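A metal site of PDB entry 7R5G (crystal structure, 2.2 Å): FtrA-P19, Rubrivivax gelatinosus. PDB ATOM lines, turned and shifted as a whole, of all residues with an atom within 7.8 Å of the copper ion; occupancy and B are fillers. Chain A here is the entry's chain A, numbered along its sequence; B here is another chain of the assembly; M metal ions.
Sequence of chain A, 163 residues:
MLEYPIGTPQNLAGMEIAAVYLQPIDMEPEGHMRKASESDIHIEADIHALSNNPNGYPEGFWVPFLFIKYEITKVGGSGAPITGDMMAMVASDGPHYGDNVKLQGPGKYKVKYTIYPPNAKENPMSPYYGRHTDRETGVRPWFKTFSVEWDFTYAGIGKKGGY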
ATOM      1  N   MET A   1      28.351 -30.632  -3.475  1.00  0.00           N
ATOM      2  CA  MET A   1      27.519 -31.076  -2.336  1.00  0.00           C
ATOM      3  C   MET A   1      26.137 -31.655  -2.743  1.00  0.00           C
ATOM      4  O   MET A   1      25.605 -31.294  -3.792  1.00  0.00           O
ATOM      5  CB  MET A   1      27.362 -29.952  -1.298  1.00  0.00           C
ATOM      6  CG  MET A   1      27.503 -30.451   0.116  1.00  0.00           C
ATOM      7  SD  MET A   1      27.731 -29.115   1.335  1.00  0.00           S
ATOM      8  CE  MET A   1      26.006 -28.807   1.767  1.00  0.00           C
ATOM      9  N   LEU A  22      19.160 -31.308   4.030  1.00  0.00           N
ATOM     10  CA  LEU A  22      20.102 -32.416   3.862  1.00  0.00           C
ATOM     11  C   LEU A  22      20.115 -33.173   5.203  1.00  0.00           C
ATOM     12  O   LEU A  22      19.299 -32.904   6.078  1.00  0.00           O
ATOM     13  CB  LEU A  22      21.502 -31.910   3.477  1.00  0.00           C
ATOM     14  CG  LEU A  22      22.096 -30.815   4.391  1.00  0.00           C
ATOM     15  CD1 LEU A  22      23.520 -31.095   4.706  1.00  0.00           C
ATOM     16  CD2 LEU A  22      21.931 -29.420   3.775  1.00  0.00           C
ATOM     17  N   GLN A  23      21.026 -34.113   5.364  1.00  0.00           N
ATOM     18  CA  GLN A  23      21.118 -34.860   6.603  1.00  0.00           C
ATOM     19  C   GLN A  23      21.558 -33.950   7.803  1.00  0.00           C
ATOM     20  O   GLN A  23      22.185 -32.917   7.580  1.00  0.00           O
ATOM     21  CB  GLN A  23      22.044 -36.091   6.393  1.00  0.00           C
ATOM     22  CG  GLN A  23      23.562 -35.801   6.441  1.00  0.00           C
ATOM     23  CD  GLN A  23      24.150 -35.089   5.242  1.00  0.00           C
ATOM     24  OE1 GLN A  23      23.533 -34.925   4.183  1.00  0.00           O
ATOM     25  NE2 GLN A  23      25.392 -34.645   5.381  1.00  0.00           N
ATOM     26  N   ILE A  25      23.757 -32.302  10.689  1.00  0.00           N
ATOM     27  CA  ILE A  25      25.204 -32.079  10.686  1.00  0.00           C
ATOM     28  C   ILE A  25      25.771 -31.876  12.071  1.00  0.00           C
ATOM     29  O   ILE A  25      25.013 -31.776  13.019  1.00  0.00           O
ATOM     30  CB  ILE A  25      25.576 -30.888   9.725  1.00  0.00           C
ATOM     31  CG1 ILE A  25      24.906 -29.555  10.095  1.00  0.00           C
ATOM     32  CG2 ILE A  25      25.258 -31.252   8.260  1.00  0.00           C
ATOM     33  CD1 ILE A  25      25.626 -28.612  11.127  1.00  0.00           C
ATOM     34  N   ASP A  26      27.118 -31.791  12.162  1.00  0.00           N
ATOM     35  CA  ASP A  26      27.917 -31.466  13.345  1.00  0.00           C
ATOM     36  C   ASP A  26      28.561 -30.086  13.086  1.00  0.00           C
ATOM     37  O   ASP A  26      28.983 -29.782  11.960  1.00  0.00           O
ATOM     38  CB  ASP A  26      29.028 -32.511  13.590  1.00  0.00           C
ATOM     39  CG  ASP A  26      28.540 -33.941  13.695  1.00  0.00           C
ATOM     40  OD1 ASP A  26      27.394 -34.158  14.158  1.00  0.00           O
ATOM     41  OD2 ASP A  26      29.300 -34.858  13.322  1.00  0.00           O
ATOM     42  N   MET A  27      28.608 -29.255  14.126  1.00  0.00           N
ATOM     43  CA  MET A  27      29.063 -27.893  13.977  1.00  0.00           C
ATOM     44  C   MET A  27      29.927 -27.454  15.157  1.00  0.00           C
ATOM     45  O   MET A  27      29.720 -27.891  16.301  1.00  0.00           O
ATOM     46  CB  MET A  27      27.818 -26.979  13.856  1.00  0.00           C
ATOM     47  CG  MET A  27      28.074 -25.583  13.272  1.00  0.00           C
ATOM     48  SD  MET A  27      26.779 -24.396  13.720  1.00  0.00           S
ATOM     49  CE  MET A  27      27.149 -24.186  15.496  1.00  0.00           C
ATOM     50  N   MET A  33      23.867 -26.427  17.913  1.00  0.00           N
ATOM     51  CA  MET A  33      22.960 -27.239  17.099  1.00  0.00           C
ATOM     52  C   MET A  33      22.384 -28.324  17.952  1.00  0.00           C
ATOM     53  O   MET A  33      23.054 -28.841  18.860  1.00  0.00           O
ATOM     54  CB  MET A  33      23.700 -27.939  15.926  1.00  0.00           C
ATOM     55  CG  MET A  33      24.130 -27.032  14.787  1.00  0.00           C
ATOM     56  SD  MET A  33      22.781 -26.374  13.788  1.00  0.00           S
ATOM     57  CE  MET A  33      22.647 -24.726  14.504  1.00  0.00           C
ATOM     58  N   HIS A  42      18.861 -31.206   8.365  1.00  0.00           N
ATOM     59  CA  HIS A  42      19.507 -29.939   8.500  1.00  0.00           C
ATOM     60  C   HIS A  42      18.755 -29.027   7.519  1.00  0.00           C
ATOM     61  O   HIS A  42      18.773 -29.282   6.320  1.00  0.00           O
ATOM     62  CB  HIS A  42      21.009 -29.977   8.196  1.00  0.00           C
ATOM     63  CG  HIS A  42      21.698 -28.688   8.508  1.00  0.00           C
ATOM     64  ND1 HIS A  42      21.781 -28.219   9.812  1.00  0.00           N
ATOM     65  CD2 HIS A  42      22.329 -27.812   7.692  1.00  0.00           C
ATOM     66  CE1 HIS A  42      22.446 -27.062   9.747  1.00  0.00           C
ATOM     67  NE2 HIS A  42      22.795 -26.782   8.486  1.00  0.00           N
ATOM     68  N   ILE A  43      17.982 -28.074   8.025  1.00  0.00           N
ATOM     69  CA  ILE A  43      17.234 -27.144   7.177  1.00  0.00           C
ATOM     70  C   ILE A  43      18.111 -25.915   6.865  1.00  0.00           C
ATOM     71  O   ILE A  43      18.864 -25.465   7.736  1.00  0.00           O
ATOM     72  CB  ILE A  43      15.812 -26.798   7.705  1.00  0.00           C
ATOM     73  CG1 ILE A  43      14.952 -26.238   6.531  1.00  0.00           C
ATOM     74  CG2 ILE A  43      15.865 -25.800   8.915  1.00  0.00           C
ATOM     75  CD1 ILE A  43      13.567 -26.570   6.515  1.00  0.00           C
ATOM     76  N   GLU A  44      18.046 -25.403   5.639  1.00  0.00           N
ATOM     77  CA  GLU A  44      18.893 -24.295   5.229  1.00  0.00           C
ATOM     78  C   GLU A  44      18.170 -23.246   4.401  1.00  0.00           C
ATOM     79  O   GLU A  44      17.221 -23.568   3.687  1.00  0.00           O
ATOM     80  CB  GLU A  44      20.109 -24.879   4.479  1.00  0.00           C
ATOM     81  CG  GLU A  44      20.945 -23.998   3.567  1.00  0.00           C
ATOM     82  CD  GLU A  44      22.020 -24.762   2.816  1.00  0.00           C
ATOM     83  OE1 GLU A  44      22.380 -25.878   3.249  1.00  0.00           O
ATOM     84  OE2 GLU A  44      22.498 -24.267   1.783  1.00  0.00           O
ATOM     85  N   MET A  87      21.049 -20.324  12.210  1.00  0.00           N
ATOM     86  CA  MET A  87      22.302 -19.711  12.597  1.00  0.00           C
ATOM     87  C   MET A  87      23.118 -19.597  11.314  1.00  0.00           C
ATOM     88  O   MET A  87      23.018 -20.477  10.465  1.00  0.00           O
ATOM     89  CB  MET A  87      22.981 -20.613  13.631  1.00  0.00           C
ATOM     90  CG  MET A  87      24.293 -20.079  14.149  1.00  0.00           C
ATOM     91  SD  MET A  87      24.993 -21.203  15.377  1.00  0.00           S
ATOM     92  CE  MET A  87      26.558 -20.280  15.743  1.00  0.00           C
ATOM     93  N   ALA A  88      23.914 -18.529  11.163  1.00  0.00           N
ATOM     94  CA  ALA A  88      24.835 -18.342  10.021  1.00  0.00           C
ATOM     95  C   ALA A  88      26.003 -19.305  10.286  1.00  0.00           C
ATOM     96  O   ALA A  88      26.417 -19.511  11.445  1.00  0.00           O
ATOM     97  CB  ALA A  88      25.345 -16.898   9.963  1.00  0.00           C
ATOM     98  N   MET A  89      26.484 -19.943   9.227  1.00  0.00           N
ATOM     99  CA  MET A  89      27.555 -20.922   9.283  1.00  0.00           C
ATOM    100  C   MET A  89      28.140 -21.187   7.910  1.00  0.00           C
ATOM    101  O   MET A  89      27.559 -20.824   6.893  1.00  0.00           O
ATOM    102  CB  MET A  89      27.080 -22.251   9.929  1.00  0.00           C
ATOM    103  CG  MET A  89      25.943 -22.906   9.204  1.00  0.00           C
ATOM    104  SD  MET A  89      25.275 -24.317  10.094  1.00  0.00           S
ATOM    105  CE  MET A  89      24.161 -23.504  11.193  1.00  0.00           C
ATOM    106  N   VAL A  90      29.283 -21.855   7.881  1.00  0.00           N
ATOM    107  CA  VAL A  90      29.936 -22.234   6.649  1.00  0.00           C
ATOM    108  C   VAL A  90      30.064 -23.756   6.556  1.00  0.00           C
ATOM    109  O   VAL A  90      30.335 -24.433   7.565  1.00  0.00           O
ATOM    110  CB  VAL A  90      31.269 -21.476   6.465  1.00  0.00           C
ATOM    111  CG1 VAL A  90      32.349 -22.001   7.401  1.00  0.00           C
ATOM    112  CG2 VAL A  90      31.712 -21.500   4.995  1.00  0.00           C
ATOM    113  N   ALA A  91      29.810 -24.287   5.337  1.00  0.00           N
ATOM    114  CA  ALA A  91      29.932 -25.716   4.994  1.00  0.00           C
ATOM    115  C   ALA A  91      30.796 -25.797   3.726  1.00  0.00           C
ATOM    116  O   ALA A  91      31.253 -24.747   3.248  1.00  0.00           O
ATOM    117  CB  ALA A  91      28.545 -26.320   4.773  1.00  0.00           C
ATOM    118  N   ASP A  93      30.199 -26.163   0.640  1.00  0.00           N
ATOM    119  CA  ASP A  93      29.641 -25.430  -0.504  1.00  0.00           C
ATOM    120  C   ASP A  93      29.526 -23.901  -0.218  1.00  0.00           C
ATOM    121  O   ASP A  93      29.007 -23.150  -1.057  1.00  0.00           O
ATOM    122  CB  ASP A  93      28.282 -26.027  -0.902  1.00  0.00           C
ATOM    123  CG  ASP A  93      27.173 -25.874   0.134  1.00  0.00           C
ATOM    124  OD1 ASP A  93      27.502 -25.741   1.365  1.00  0.00           O
ATOM    125  OD2 ASP A  93      25.978 -25.911  -0.254  1.00  0.00           O
ATOM    126  N   GLY A  94      29.976 -23.472   0.966  1.00  0.00           N
ATOM    127  CA  GLY A  94      29.940 -22.065   1.340  1.00  0.00           C
ATOM    128  C   GLY A  94      29.050 -21.692   2.521  1.00  0.00           C
ATOM    129  O   GLY A  94      28.450 -22.563   3.183  1.00  0.00           O
ATOM    130  N   PRO A  95      28.979 -20.377   2.800  1.00  0.00           N
ATOM    131  CA  PRO A  95      28.158 -19.898   3.919  1.00  0.00           C
ATOM    132  C   PRO A  95      26.651 -19.941   3.631  1.00  0.00           C
ATOM    133  O   PRO A  95      26.199 -19.795   2.488  1.00  0.00           O
ATOM    134  CB  PRO A  95      28.678 -18.474   4.114  1.00  0.00           C
ATOM    135  CG  PRO A  95      29.031 -18.036   2.696  1.00  0.00           C
ATOM    136  CD  PRO A  95      29.625 -19.254   2.083  1.00  0.00           C
ATOM    137  N   HIS A  96      25.886 -20.198   4.675  1.00  0.00           N
ATOM    138  CA  HIS A  96      24.426 -20.287   4.622  1.00  0.00           C
ATOM    139  C   HIS A  96      23.850 -20.067   6.033  1.00  0.00           C
ATOM    140  O   HIS A  96      24.600 -19.869   6.972  1.00  0.00           O
ATOM    141  CB  HIS A  96      24.005 -21.680   4.029  1.00  0.00           C
ATOM    142  CG  HIS A  96      24.392 -22.816   4.920  1.00  0.00           C
ATOM    143  ND1 HIS A  96      25.664 -23.351   4.908  1.00  0.00           N
ATOM    144  CD2 HIS A  96      23.679 -23.411   5.908  1.00  0.00           C
ATOM    145  CE1 HIS A  96      25.691 -24.266   5.853  1.00  0.00           C
ATOM    146  NE2 HIS A  96      24.516 -24.351   6.481  1.00  0.00           N
ATOM    147  N   TYR A  97      22.514 -20.141   6.164  1.00  0.00           N
ATOM    148  CA  TYR A  97      21.759 -20.081   7.415  1.00  0.00           C
ATOM    149  C   TYR A  97      21.130 -21.453   7.536  1.00  0.00           C
ATOM    150  O   TYR A  97      20.570 -21.957   6.559  1.00  0.00           O
ATOM    151  CB  TYR A  97      20.704 -18.963   7.385  1.00  0.00           C
ATOM    152  CG  TYR A  97      21.310 -17.605   7.122  1.00  0.00           C
ATOM    153  CD1 TYR A  97      21.891 -16.861   8.138  1.00  0.00           C
ATOM    154  CD2 TYR A  97      21.283 -17.051   5.842  1.00  0.00           C
ATOM    155  CE1 TYR A  97      22.470 -15.611   7.898  1.00  0.00           C
ATOM    156  CE2 TYR A  97      21.874 -15.819   5.578  1.00  0.00           C
ATOM    157  CZ  TYR A  97      22.412 -15.079   6.621  1.00  0.00           C
ATOM    158  OH  TYR A  97      23.022 -13.879   6.357  1.00  0.00           O
ATOM    159  N   GLY A  98      21.314 -22.102   8.692  1.00  0.00           N
ATOM    160  CA  GLY A  98      20.795 -23.437   8.886  1.00  0.00           C
ATOM    161  C   GLY A  98      20.500 -23.836  10.314  1.00  0.00           C
ATOM    162  O   GLY A  98      20.864 -23.151  11.265  1.00  0.00           O
ATOM    163  N   ASP A  99      19.834 -24.986  10.462  1.00  0.00           N
ATOM    164  CA  ASP A  99      19.490 -25.550  11.760  1.00  0.00           C
ATOM    165  C   ASP A  99      19.180 -27.028  11.661  1.00  0.00           C
ATOM    166  O   ASP A  99      18.574 -27.448  10.691  1.00  0.00           O
ATOM    167  CB  ASP A  99      18.304 -24.800  12.411  1.00  0.00           C
ATOM    168  CG  ASP A  99      18.303 -24.895  13.932  1.00  0.00           C
ATOM    169  OD1 ASP A  99      19.409 -24.921  14.520  1.00  0.00           O
ATOM    170  OD2 ASP A  99      17.197 -24.927  14.532  1.00  0.00           O
ATOM    171  N   ASN A 100      19.590 -27.823  12.675  1.00  0.00           N
ATOM    172  CA  ASN A 100      19.206 -29.239  12.778  1.00  0.00           C
ATOM    173  C   ASN A 100      17.806 -29.249  13.361  1.00  0.00           C
ATOM    174  O   ASN A 100      17.537 -28.540  14.339  1.00  0.00           O
ATOM    175  CB  ASN A 100      20.164 -30.031  13.676  1.00  0.00           C
ATOM    176  CG  ASN A 100      21.437 -30.450  12.993  1.00  0.00           C
ATOM    177  OD1 ASN A 100      21.693 -30.124  11.815  1.00  0.00           O
ATOM    178  ND2 ASN A 100      22.270 -31.151  13.725  1.00  0.00           N
ATOM    179  N   GLY B 130      28.890 -20.378  12.759  1.00  0.00           N
ATOM    180  CA  GLY B 130      29.315 -21.767  12.898  1.00  0.00           C
ATOM    181  C   GLY B 130      30.180 -22.278  11.754  1.00  0.00           C
ATOM    182  O   GLY B 130      30.475 -21.572  10.790  1.00  0.00           O
ATOM    183  N   ARG B 131      30.566 -23.535  11.860  1.00  0.00           N
ATOM    184  CA  ARG B 131      31.400 -24.227  10.901  1.00  0.00           C
ATOM    185  C   ARG B 131      31.030 -25.703  10.970  1.00  0.00           C
ATOM    186  O   ARG B 131      31.170 -26.323  12.026  1.00  0.00           O
ATOM    187  CB  ARG B 131      32.890 -24.008  11.284  1.00  0.00           C
ATOM    188  CG  ARG B 131      33.885 -24.820  10.488  1.00  0.00           C
ATOM    189  CD  ARG B 131      35.322 -24.527  10.900  1.00  0.00           C
ATOM    190  NE  ARG B 131      35.721 -25.254  12.109  1.00  0.00           N
ATOM    191  CZ  ARG B 131      36.139 -26.512  12.145  1.00  0.00           C
ATOM    192  NH1 ARG B 131      36.185 -27.239  11.034  1.00  0.00           N
ATOM    193  NH2 ARG B 131      36.481 -27.064  13.294  1.00  0.00           N
ATOM    194  N   HIS B 132      30.614 -26.288   9.838  1.00  0.00           N
ATOM    195  CA  HIS B 132      30.336 -27.717   9.746  1.00  0.00           C
ATOM    196  C   HIS B 132      31.632 -28.492   9.969  1.00  0.00           C
ATOM    197  O   HIS B 132      32.685 -28.094   9.452  1.00  0.00           O
ATOM    198  CB  HIS B 132      29.718 -28.107   8.399  1.00  0.00           C
ATOM    199  CG  HIS B 132      28.294 -27.693   8.207  1.00  0.00           C
ATOM    200  ND1 HIS B 132      27.413 -28.479   7.490  1.00  0.00           N
ATOM    201  CD2 HIS B 132      27.660 -26.572   8.594  1.00  0.00           C
ATOM    202  CE1 HIS B 132      26.286 -27.794   7.446  1.00  0.00           C
ATOM    203  NE2 HIS B 132      26.388 -26.645   8.116  1.00  0.00           N
ATOM    204  N   ASP B 134      31.400 -32.295  10.167  1.00  0.00           N
ATOM    205  CA  ASP B 134      31.118 -33.681   9.730  1.00  0.00           C
ATOM    206  C   ASP B 134      31.843 -33.980   8.409  1.00  0.00           C
ATOM    207  O   ASP B 134      32.211 -33.058   7.698  1.00  0.00           O
ATOM    208  CB  ASP B 134      29.609 -33.903   9.586  1.00  0.00           C
ATOM    209  CG  ASP B 134      28.934 -32.868   8.700  1.00  0.00           C
ATOM    210  OD1 ASP B 134      28.706 -31.718   9.184  1.00  0.00           O
ATOM    211  OD2 ASP B 134      28.656 -33.176   7.522  1.00  0.00           O
ATOM    212  N   THR B 137      29.823 -32.649   4.770  1.00  0.00           N
ATOM    213  CA  THR B 137      29.675 -31.210   4.517  1.00  0.00           C
ATOM    214  C   THR B 137      30.682 -30.322   5.259  1.00  0.00           C
ATOM    215  O   THR B 137      30.659 -29.111   5.090  1.00  0.00           O
ATOM    216  CB  THR B 137      28.223 -30.786   4.819  1.00  0.00           C
ATOM    217  OG1 THR B 137      28.000 -30.829   6.227  1.00  0.00           O
ATOM    218  CG2 THR B 137      27.178 -31.654   4.084  1.00  0.00           C
HETATM  219 CU    CU M   1      24.521 -25.529   8.242  1.00  0.00          CU
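The copper ion is bound by NE2 of His 96 (2.1 Å), NE2 of His 42 (2.1 Å), NE2 of His 132 of chain B (2.2 Å) and SD of Met 89 (2.3 Å). The copper ion has four donor atoms within binding distance.
Of the 28 residues printed, 4 come within 4 Å of the copper ion.
The backbone carbonyl oxygen of Gly 94 is in hydrogen-bond range of a ring nitrogen (ND1) of His 96. A ring nitrogen (ND1) of His 132 of chain B lies within hydrogen-bond range of the side-chain hydroxyl (OG1) of Thr 137 of chain B. N of His 42 sits at hydrogen-bond distance from O of Leu 22 (2.9 Å). A ring nitrogen (ND1) of His 42 sits close to the backbone carbonyl oxygen (O) of Asp 99 (3.4 Å). A ring nitrogen (ND1) of His 42 lies within hydrogen-bond range of the side-chain amide oxygen of Asn 100 (2.8 Å). The backbone carbonyl oxygen (O) of Val 90 lies within hydrogen-bond range of the backbone NH (N) of His 132 of chain B, 2.9 Å away.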
